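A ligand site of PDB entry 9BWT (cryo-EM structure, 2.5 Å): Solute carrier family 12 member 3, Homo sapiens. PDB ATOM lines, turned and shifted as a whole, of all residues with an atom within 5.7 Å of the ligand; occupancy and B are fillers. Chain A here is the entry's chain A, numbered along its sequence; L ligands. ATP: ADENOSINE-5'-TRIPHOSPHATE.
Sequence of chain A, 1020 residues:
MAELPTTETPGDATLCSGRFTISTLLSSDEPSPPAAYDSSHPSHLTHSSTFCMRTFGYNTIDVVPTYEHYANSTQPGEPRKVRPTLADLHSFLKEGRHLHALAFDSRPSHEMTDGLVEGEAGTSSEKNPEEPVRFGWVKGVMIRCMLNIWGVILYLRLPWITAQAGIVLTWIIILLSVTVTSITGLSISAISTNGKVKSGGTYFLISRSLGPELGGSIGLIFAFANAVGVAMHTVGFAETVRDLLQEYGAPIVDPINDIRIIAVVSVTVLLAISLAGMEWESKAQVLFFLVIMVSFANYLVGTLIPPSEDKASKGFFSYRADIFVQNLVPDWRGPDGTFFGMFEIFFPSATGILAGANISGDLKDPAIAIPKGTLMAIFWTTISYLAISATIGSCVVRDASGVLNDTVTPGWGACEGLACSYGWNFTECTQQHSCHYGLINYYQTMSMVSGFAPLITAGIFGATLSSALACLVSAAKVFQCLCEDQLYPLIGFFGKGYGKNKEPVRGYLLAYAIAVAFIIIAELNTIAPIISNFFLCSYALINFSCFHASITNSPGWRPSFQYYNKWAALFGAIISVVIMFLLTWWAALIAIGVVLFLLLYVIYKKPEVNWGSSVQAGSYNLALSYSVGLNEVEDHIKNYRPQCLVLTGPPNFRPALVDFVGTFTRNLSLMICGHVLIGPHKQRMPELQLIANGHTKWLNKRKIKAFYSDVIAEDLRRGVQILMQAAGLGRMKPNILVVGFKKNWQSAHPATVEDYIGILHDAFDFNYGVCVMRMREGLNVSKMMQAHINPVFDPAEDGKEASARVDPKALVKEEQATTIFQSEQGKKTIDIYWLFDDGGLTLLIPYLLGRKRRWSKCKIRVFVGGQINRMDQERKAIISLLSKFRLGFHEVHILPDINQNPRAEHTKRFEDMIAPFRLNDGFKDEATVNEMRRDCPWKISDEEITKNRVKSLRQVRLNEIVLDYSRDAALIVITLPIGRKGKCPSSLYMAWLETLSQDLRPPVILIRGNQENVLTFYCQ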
ATOM      1  N   LEU A 647     -28.987   1.228  -1.505  1.00  0.00           N
ATOM      2  CA  LEU A 647     -27.946   0.575  -0.719  1.00  0.00           C
ATOM      3  C   LEU A 647     -28.119   0.997   0.728  1.00  0.00           C
ATOM      4  O   LEU A 647     -27.640   2.050   1.143  1.00  0.00           O
ATOM      5  CB  LEU A 647     -26.560   0.918  -1.243  1.00  0.00           C
ATOM      6  CG  LEU A 647     -26.328   0.628  -2.721  1.00  0.00           C
ATOM      7  CD1 LEU A 647     -25.229   1.521  -3.251  1.00  0.00           C
ATOM      8  CD2 LEU A 647     -25.986  -0.833  -2.918  1.00  0.00           C
ATOM      9  N   THR A 648     -28.811   0.172   1.510  1.00  0.00           N
ATOM     10  CA  THR A 648     -29.118   0.478   2.898  1.00  0.00           C
ATOM     11  C   THR A 648     -28.408  -0.414   3.895  1.00  0.00           C
ATOM     12  O   THR A 648     -28.506  -0.173   5.092  1.00  0.00           O
ATOM     13  CB  THR A 648     -30.623   0.387   3.135  1.00  0.00           C
ATOM     14  OG1 THR A 648     -31.055  -0.971   2.948  1.00  0.00           O
ATOM     15  CG2 THR A 648     -31.378   1.269   2.175  1.00  0.00           C
ATOM     16  N   GLY A 649     -27.690  -1.435   3.429  1.00  0.00           N
ATOM     17  CA  GLY A 649     -27.195  -2.447   4.328  1.00  0.00           C
ATOM     18  C   GLY A 649     -28.360  -3.070   5.069  1.00  0.00           C
ATOM     19  O   GLY A 649     -29.403  -3.355   4.483  1.00  0.00           O
ATOM     20  N   PRO A 650     -28.213  -3.268   6.375  1.00  0.00           N
ATOM     21  CA  PRO A 650     -29.354  -3.690   7.177  1.00  0.00           C
ATOM     22  C   PRO A 650     -30.404  -2.596   7.195  1.00  0.00           C
ATOM     23  O   PRO A 650     -30.134  -1.480   7.653  1.00  0.00           O
ATOM     24  CB  PRO A 650     -28.750  -3.911   8.572  1.00  0.00           C
ATOM     25  CG  PRO A 650     -27.277  -3.991   8.355  1.00  0.00           C
ATOM     26  CD  PRO A 650     -26.998  -3.125   7.181  1.00  0.00           C
ATOM     27  N   ARG A 654     -30.313   2.148   8.577  1.00  0.00           N
ATOM     28  CA  ARG A 654     -30.504   3.434   7.925  1.00  0.00           C
ATOM     29  C   ARG A 654     -31.951   3.536   7.472  1.00  0.00           C
ATOM     30  O   ARG A 654     -32.250   3.331   6.281  1.00  0.00           O
ATOM     31  CB  ARG A 654     -29.548   3.613   6.749  1.00  0.00           C
ATOM     32  CG  ARG A 654     -28.084   3.500   7.124  1.00  0.00           C
ATOM     33  CD  ARG A 654     -27.246   3.105   5.926  1.00  0.00           C
ATOM     34  NE  ARG A 654     -25.838   3.000   6.280  1.00  0.00           N
ATOM     35  CZ  ARG A 654     -25.213   1.854   6.504  1.00  0.00           C
ATOM     36  NH1 ARG A 654     -25.834   0.700   6.409  1.00  0.00           N
ATOM     37  NH2 ARG A 654     -23.917   1.875   6.829  1.00  0.00           N
ATOM     38  N   LEU A 657     -33.087   6.442   4.645  1.00  0.00           N
ATOM     39  CA  LEU A 657     -32.950   6.129   3.228  1.00  0.00           C
ATOM     40  C   LEU A 657     -34.161   5.359   2.720  1.00  0.00           C
ATOM     41  O   LEU A 657     -34.746   5.705   1.672  1.00  0.00           O
ATOM     42  CB  LEU A 657     -31.669   5.332   3.006  1.00  0.00           C
ATOM     43  CG  LEU A 657     -30.875   5.565   1.740  1.00  0.00           C
ATOM     44  CD1 LEU A 657     -30.602   7.043   1.551  1.00  0.00           C
ATOM     45  CD2 LEU A 657     -29.583   4.791   1.809  1.00  0.00           C
ATOM     46  N   GLY A 674     -30.732  -3.101  -0.983  1.00  0.00           N
ATOM     47  CA  GLY A 674     -29.546  -3.931  -1.144  1.00  0.00           C
ATOM     48  C   GLY A 674     -28.684  -3.934   0.099  1.00  0.00           C
ATOM     49  O   GLY A 674     -28.392  -2.886   0.682  1.00  0.00           O
ATOM     50  N   HIS A 675     -28.260  -5.125   0.505  1.00  0.00           N
ATOM     51  CA  HIS A 675     -27.405  -5.300   1.671  1.00  0.00           C
ATOM     52  C   HIS A 675     -26.250  -6.204   1.277  1.00  0.00           C
ATOM     53  O   HIS A 675     -26.465  -7.299   0.754  1.00  0.00           O
ATOM     54  CB  HIS A 675     -28.194  -5.904   2.844  1.00  0.00           C
ATOM     55  CG  HIS A 675     -27.356  -6.149   4.068  1.00  0.00           C
ATOM     56  ND1 HIS A 675     -27.738  -7.031   5.056  1.00  0.00           N
ATOM     57  CD2 HIS A 675     -26.178  -5.631   4.457  1.00  0.00           C
ATOM     58  CE1 HIS A 675     -26.825  -7.036   6.010  1.00  0.00           C
ATOM     59  NE2 HIS A 675     -25.863  -6.205   5.664  1.00  0.00           N
ATOM     60  N   VAL A 676     -25.031  -5.747   1.533  1.00  0.00           N
ATOM     61  CA  VAL A 676     -23.823  -6.479   1.179  1.00  0.00           C
ATOM     62  C   VAL A 676     -23.169  -6.960   2.464  1.00  0.00           C
ATOM     63  O   VAL A 676     -22.910  -6.168   3.374  1.00  0.00           O
ATOM     64  CB  VAL A 676     -22.852  -5.614   0.358  1.00  0.00           C
ATOM     65  CG1 VAL A 676     -21.581  -6.382   0.069  1.00  0.00           C
ATOM     66  CG2 VAL A 676     -23.509  -5.163  -0.918  1.00  0.00           C
ATOM     67  N   LEU A 677     -22.908  -8.260   2.535  1.00  0.00           N
ATOM     68  CA  LEU A 677     -22.214  -8.862   3.665  1.00  0.00           C
ATOM     69  C   LEU A 677     -20.780  -9.156   3.254  1.00  0.00           C
ATOM     70  O   LEU A 677     -20.555  -9.910   2.293  1.00  0.00           O
ATOM     71  CB  LEU A 677     -22.913 -10.132   4.126  1.00  0.00           C
ATOM     72  CG  LEU A 677     -24.431 -10.014   4.316  1.00  0.00           C
ATOM     73  CD1 LEU A 677     -25.086 -11.361   4.071  1.00  0.00           C
ATOM     74  CD2 LEU A 677     -24.745  -9.507   5.702  1.00  0.00           C
ATOM     75  N   ILE A 678     -19.816  -8.582   3.970  1.00  0.00           N
ATOM     76  CA  ILE A 678     -18.411  -8.816   3.634  1.00  0.00           C
ATOM     77  C   ILE A 678     -18.092 -10.305   3.684  1.00  0.00           C
ATOM     78  O   ILE A 678     -17.701 -10.914   2.687  1.00  0.00           O
ATOM     79  CB  ILE A 678     -17.492  -8.001   4.568  1.00  0.00           C
ATOM     80  CG1 ILE A 678     -17.349  -6.571   4.067  1.00  0.00           C
ATOM     81  CG2 ILE A 678     -16.134  -8.671   4.682  1.00  0.00           C
ATOM     82  CD1 ILE A 678     -18.657  -5.902   3.696  1.00  0.00           C
ATOM     83  N   LEU A 716     -17.536  -3.800  -0.300  1.00  0.00           N
ATOM     84  CA  LEU A 716     -18.824  -3.220  -0.654  1.00  0.00           C
ATOM     85  C   LEU A 716     -18.955  -3.014  -2.156  1.00  0.00           C
ATOM     86  O   LEU A 716     -20.026  -3.229  -2.730  1.00  0.00           O
ATOM     87  CB  LEU A 716     -19.015  -1.897   0.085  1.00  0.00           C
ATOM     88  CG  LEU A 716     -20.346  -1.177  -0.136  1.00  0.00           C
ATOM     89  CD1 LEU A 716     -21.485  -1.981   0.465  1.00  0.00           C
ATOM     90  CD2 LEU A 716     -20.305   0.213   0.453  1.00  0.00           C
ATOM     91  N   VAL A 738     -29.422   4.527  -5.356  1.00  0.00           N
ATOM     92  CA  VAL A 738     -29.587   5.466  -4.257  1.00  0.00           C
ATOM     93  C   VAL A 738     -28.653   5.033  -3.137  1.00  0.00           C
ATOM     94  O   VAL A 738     -28.829   3.963  -2.552  1.00  0.00           O
ATOM     95  CB  VAL A 738     -31.052   5.509  -3.761  1.00  0.00           C
ATOM     96  CG1 VAL A 738     -31.231   6.626  -2.763  1.00  0.00           C
ATOM     97  CG2 VAL A 738     -31.989   5.681  -4.935  1.00  0.00           C
ATOM     98  N   VAL A 739     -27.676   5.872  -2.840  1.00  0.00           N
ATOM     99  CA  VAL A 739     -26.665   5.571  -1.831  1.00  0.00           C
ATOM    100  C   VAL A 739     -26.535   6.768  -0.903  1.00  0.00           C
ATOM    101  O   VAL A 739     -26.748   7.916  -1.297  1.00  0.00           O
ATOM    102  CB  VAL A 739     -25.306   5.221  -2.471  1.00  0.00           C
ATOM    103  CG1 VAL A 739     -24.761   6.422  -3.210  1.00  0.00           C
ATOM    104  CG2 VAL A 739     -24.337   4.759  -1.413  1.00  0.00           C
ATOM    105  N   GLY A 740     -26.181   6.486   0.339  1.00  0.00           N
ATOM    106  CA  GLY A 740     -25.987   7.546   1.311  1.00  0.00           C
ATOM    107  C   GLY A 740     -24.625   8.193   1.204  1.00  0.00           C
ATOM    108  O   GLY A 740     -23.685   7.649   0.627  1.00  0.00           O
ATOM    109  N   PHE A 741     -24.522   9.395   1.761  1.00  0.00           N
ATOM    110  CA  PHE A 741     -23.264  10.101   1.819  1.00  0.00           C
ATOM    111  C   PHE A 741     -22.421   9.565   2.970  1.00  0.00           C
ATOM    112  O   PHE A 741     -22.938   9.371   4.080  1.00  0.00           O
ATOM    113  CB  PHE A 741     -23.499  11.596   1.980  1.00  0.00           C
ATOM    114  CG  PHE A 741     -22.258  12.430   1.893  1.00  0.00           C
ATOM    115  CD1 PHE A 741     -21.715  12.764   0.664  1.00  0.00           C
ATOM    116  CD2 PHE A 741     -21.621  12.877   3.034  1.00  0.00           C
ATOM    117  CE1 PHE A 741     -20.579  13.524   0.582  1.00  0.00           C
ATOM    118  CE2 PHE A 741     -20.485  13.637   2.952  1.00  0.00           C
ATOM    119  CZ  PHE A 741     -19.955  13.961   1.729  1.00  0.00           C
ATOM    120  N   LYS A 742     -21.141   9.318   2.716  1.00  0.00           N
ATOM    121  CA  LYS A 742     -20.241   8.843   3.760  1.00  0.00           C
ATOM    122  C   LYS A 742     -19.551  10.056   4.368  1.00  0.00           C
ATOM    123  O   LYS A 742     -18.541  10.536   3.869  1.00  0.00           O
ATOM    124  CB  LYS A 742     -19.249   7.821   3.212  1.00  0.00           C
ATOM    125  CG  LYS A 742     -18.287   8.363   2.186  1.00  0.00           C
ATOM    126  CD  LYS A 742     -17.122   7.401   2.007  1.00  0.00           C
ATOM    127  CE  LYS A 742     -16.666   6.864   3.349  1.00  0.00           C
ATOM    128  NZ  LYS A 742     -15.625   5.809   3.201  1.00  0.00           N
ATOM    129  N   LYS A 743     -20.121  10.560   5.460  1.00  0.00           N
ATOM    130  CA  LYS A 743     -19.602  11.777   6.071  1.00  0.00           C
ATOM    131  C   LYS A 743     -18.297  11.563   6.814  1.00  0.00           C
ATOM    132  O   LYS A 743     -17.663  12.541   7.221  1.00  0.00           O
ATOM    133  CB  LYS A 743     -20.638  12.362   7.028  1.00  0.00           C
ATOM    134  CG  LYS A 743     -21.017  11.472   8.188  1.00  0.00           C
ATOM    135  CD  LYS A 743     -21.118  12.275   9.480  1.00  0.00           C
ATOM    136  CE  LYS A 743     -21.663  11.450  10.622  1.00  0.00           C
ATOM    137  NZ  LYS A 743     -23.149  11.467  10.643  1.00  0.00           N
ATOM    138  N   ASN A 744     -17.853  10.310   6.993  1.00  0.00           N
ATOM    139  CA  ASN A 744     -16.613  10.003   7.691  1.00  0.00           C
ATOM    140  C   ASN A 744     -15.441   9.833   6.751  1.00  0.00           C
ATOM    141  O   ASN A 744     -14.396   9.305   7.157  1.00  0.00           O
ATOM    142  CB  ASN A 744     -16.805   8.756   8.546  1.00  0.00           C
ATOM    143  CG  ASN A 744     -16.853   7.493   7.722  1.00  0.00           C
ATOM    144  OD1 ASN A 744     -15.818   6.915   7.391  1.00  0.00           O
ATOM    145  ND2 ASN A 744     -18.051   7.055   7.378  1.00  0.00           N
ATOM    146  N   THR A 752     -11.175   3.323   1.351  1.00  0.00           N
ATOM    147  CA  THR A 752     -12.636   3.283   1.487  1.00  0.00           C
ATOM    148  C   THR A 752     -13.291   4.339   0.615  1.00  0.00           C
ATOM    149  O   THR A 752     -14.285   4.054  -0.080  1.00  0.00           O
ATOM    150  CB  THR A 752     -13.028   3.467   2.950  1.00  0.00           C
ATOM    151  OG1 THR A 752     -12.040   2.852   3.792  1.00  0.00           O
ATOM    152  CG2 THR A 752     -14.376   2.842   3.222  1.00  0.00           C
ATOM    153  N   TYR A 756     -15.810   3.939  -2.548  1.00  0.00           N
ATOM    154  CA  TYR A 756     -17.090   4.642  -2.644  1.00  0.00           C
ATOM    155  C   TYR A 756     -17.227   5.361  -3.978  1.00  0.00           C
ATOM    156  O   TYR A 756     -18.228   5.216  -4.697  1.00  0.00           O
ATOM    157  CB  TYR A 756     -17.198   5.624  -1.472  1.00  0.00           C
ATOM    158  CG  TYR A 756     -18.540   6.308  -1.336  1.00  0.00           C
ATOM    159  CD1 TYR A 756     -19.554   5.731  -0.604  1.00  0.00           C
ATOM    160  CD2 TYR A 756     -18.759   7.554  -1.902  1.00  0.00           C
ATOM    161  CE1 TYR A 756     -20.779   6.359  -0.458  1.00  0.00           C
ATOM    162  CE2 TYR A 756     -19.972   8.193  -1.762  1.00  0.00           C
ATOM    163  CZ  TYR A 756     -20.972   7.586  -1.037  1.00  0.00           C
ATOM    164  OH  TYR A 756     -22.185   8.225  -0.897  1.00  0.00           O
ATOM    165  N   GLY A 778     -26.110  11.909   9.691  1.00  0.00           N
ATOM    166  CA  GLY A 778     -25.788  10.613   9.115  1.00  0.00           C
ATOM    167  C   GLY A 778     -27.000   9.717   9.010  1.00  0.00           C
ATOM    168  O   GLY A 778     -28.066   9.966   9.585  1.00  0.00           O
ATOM    169  N   LEU A 779     -26.837   8.653   8.229  1.00  0.00           N
ATOM    170  CA  LEU A 779     -27.926   7.710   8.020  1.00  0.00           C
ATOM    171  C   LEU A 779     -27.926   6.572   9.040  1.00  0.00           C
ATOM    172  O   LEU A 779     -28.988   6.058   9.393  1.00  0.00           O
ATOM    173  CB  LEU A 779     -27.862   7.134   6.599  1.00  0.00           C
ATOM    174  CG  LEU A 779     -28.414   8.011   5.488  1.00  0.00           C
ATOM    175  CD1 LEU A 779     -29.715   8.640   5.905  1.00  0.00           C
ATOM    176  CD2 LEU A 779     -27.397   9.084   5.109  1.00  0.00           C
ATOM    177  N   ASN A 780     -26.754   6.190   9.522  1.00  0.00           N
ATOM    178  CA  ASN A 780     -26.651   5.054  10.430  1.00  0.00           C
ATOM    179  C   ASN A 780     -27.131   5.445  11.819  1.00  0.00           C
ATOM    180  O   ASN A 780     -26.537   6.315  12.467  1.00  0.00           O
ATOM    181  CB  ASN A 780     -25.216   4.556  10.486  1.00  0.00           C
ATOM    182  CG  ASN A 780     -25.119   3.082  10.797  1.00  0.00           C
ATOM    183  OD1 ASN A 780     -26.076   2.474  11.283  1.00  0.00           O
ATOM    184  ND2 ASN A 780     -23.968   2.490  10.528  1.00  0.00           N
HETATM  185  PG  ATP L   1     -23.583   5.687   7.428  1.00  0.00           P
HETATM  186  O1G ATP L   1     -23.246   4.569   8.334  1.00  0.00           O
HETATM  187  O2G ATP L   1     -24.873   5.409   6.520  1.00  0.00           O
HETATM  188  O3G ATP L   1     -23.590   7.127   8.148  1.00  0.00           O
HETATM  189  PB  ATP L   1     -20.865   5.869   6.998  1.00  0.00           P
HETATM  190  O1B ATP L   1     -20.686   4.718   8.113  1.00  0.00           O
HETATM  191  O2B ATP L   1     -20.641   7.282   7.344  1.00  0.00           O
HETATM  192  O3B ATP L   1     -22.356   5.728   6.401  1.00  0.00           O
HETATM  193  PA  ATP L   1     -19.988   4.025   5.112  1.00  0.00           P
HETATM  194  O1A ATP L   1     -20.094   2.986   6.328  1.00  0.00           O
HETATM  195  O2A ATP L   1     -18.913   3.931   4.106  1.00  0.00           O
HETATM  196  O3A ATP L   1     -19.951   5.505   5.732  1.00  0.00           O
HETATM  197  O5' ATP L   1     -21.386   4.005   4.326  1.00  0.00           O
HETATM  198  C5' ATP L   1     -21.623   4.975   3.307  1.00  0.00           C
HETATM  199  C4' ATP L   1     -22.825   4.561   2.463  1.00  0.00           C
HETATM  200  O4' ATP L   1     -22.582   3.291   1.838  1.00  0.00           O
HETATM  201  C3' ATP L   1     -24.075   4.407   3.301  1.00  0.00           C
HETATM  202  O3' ATP L   1     -24.933   5.545   3.164  1.00  0.00           O
HETATM  203  C2' ATP L   1     -24.756   3.165   2.791  1.00  0.00           C
HETATM  204  O2' ATP L   1     -25.904   3.504   2.009  1.00  0.00           O
HETATM  205  C1' ATP L   1     -23.734   2.440   1.946  1.00  0.00           C
HETATM  206  N9  ATP L   1     -23.376   1.161   2.604  1.00  0.00           N
HETATM  207  C8  ATP L   1     -22.477   1.015   3.584  1.00  0.00           C
HETATM  208  N7  ATP L   1     -22.422  -0.290   3.933  1.00  0.00           N
HETATM  209  C5  ATP L   1     -23.296  -0.951   3.153  1.00  0.00           C
HETATM  210  C6  ATP L   1     -23.667  -2.277   3.062  1.00  0.00           C
HETATM  211  N6  ATP L   1     -23.061  -3.265   3.916  1.00  0.00           N
HETATM  212  N1  ATP L   1     -24.606  -2.642   2.163  1.00  0.00           N
HETATM  213  C2  ATP L   1     -25.176  -1.731   1.365  1.00  0.00           C
HETATM  214  N3  ATP L   1     -24.831  -0.447   1.446  1.00  0.00           N
HETATM  215  C4  ATP L   1     -23.900  -0.032   2.332  1.00  0.00           C
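N of Leu 647 sits at hydrogen-bond distance from O of Val 738 (2.9 Å). NH1 of Arg 654 lies within hydrogen-bond range of O of Thr 648 (3.1 Å). N of Gly 649 sits at hydrogen-bond distance from O of Gly 674, at 3.2 Å. N of Thr 648 sits at hydrogen-bond distance from O of Gly 674.
The backbone carbonyl oxygen of Leu 647 lies within hydrogen-bond range of an oxygen (O2') of the ligand, at 2.4 Å. O2B of the ligand sits at hydrogen-bond distance from ND2 of Asn 744, at 2.6 Å. The guanidinium group (NE) of Arg 654 is in salt-bridge range of an oxygen (O2G) of the ligand (2.6 Å). An oxygen (O1G) of the ligand lies close to the side-chain amide nitrogen of Asn 780. O3' of the ligand lies close to N of Gly 740, 3.2 Å away. A nitrogen (N1) of the ligand is in hydrogen-bond range of the backbone NH (N) of Val 676, at 3.2 Å. The backbone carbonyl oxygen of Val 676 sits at hydrogen-bond distance from a nitrogen (N6) of the ligand, 3.0 Å away. O2A of the ligand lies within salt-bridge range of NZ of Lys 742, 3.9 Å away.
Gly 649 touches the ligand. CD2 of Leu 657 touches O2' of the ligand, at 3.9 Å. O of Gly 674 touches C2 of the ligand, at 3.5 Å. His 675 touches the ligand (CA to N1, 3.9 Å). CD1 of Leu 716 touches C5 of the ligand (3.4 Å). Val 739 touches the ligand (CG2 to O2', 3.97 Å). N of Lys 743 touches O2B of the ligand (3.8 Å). CE1 of Tyr 756 touches C4' of the ligand, 3.99 Å away. CB of Leu 779 touches O2G of the ligand (3.5 Å). Hydrophobic or aromatic side chains that line the ligand: Leu 647, Leu 657, His 675, Val 676, Leu 716, Val 739, Tyr 756 and Leu 779. 16 residues have an atom within 4 Å of the ligand: Leu 647, Gly 649, Arg 654, Leu 657, Gly 674, His 675, Val 676, Leu 716, Val 739, Gly 740, Lys 742, Lys 743, Asn 744, Tyr 756, Leu 779 and Asn 780. The nearest printed residue that does not touch the ligand is Thr 648 (4.03 Å).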
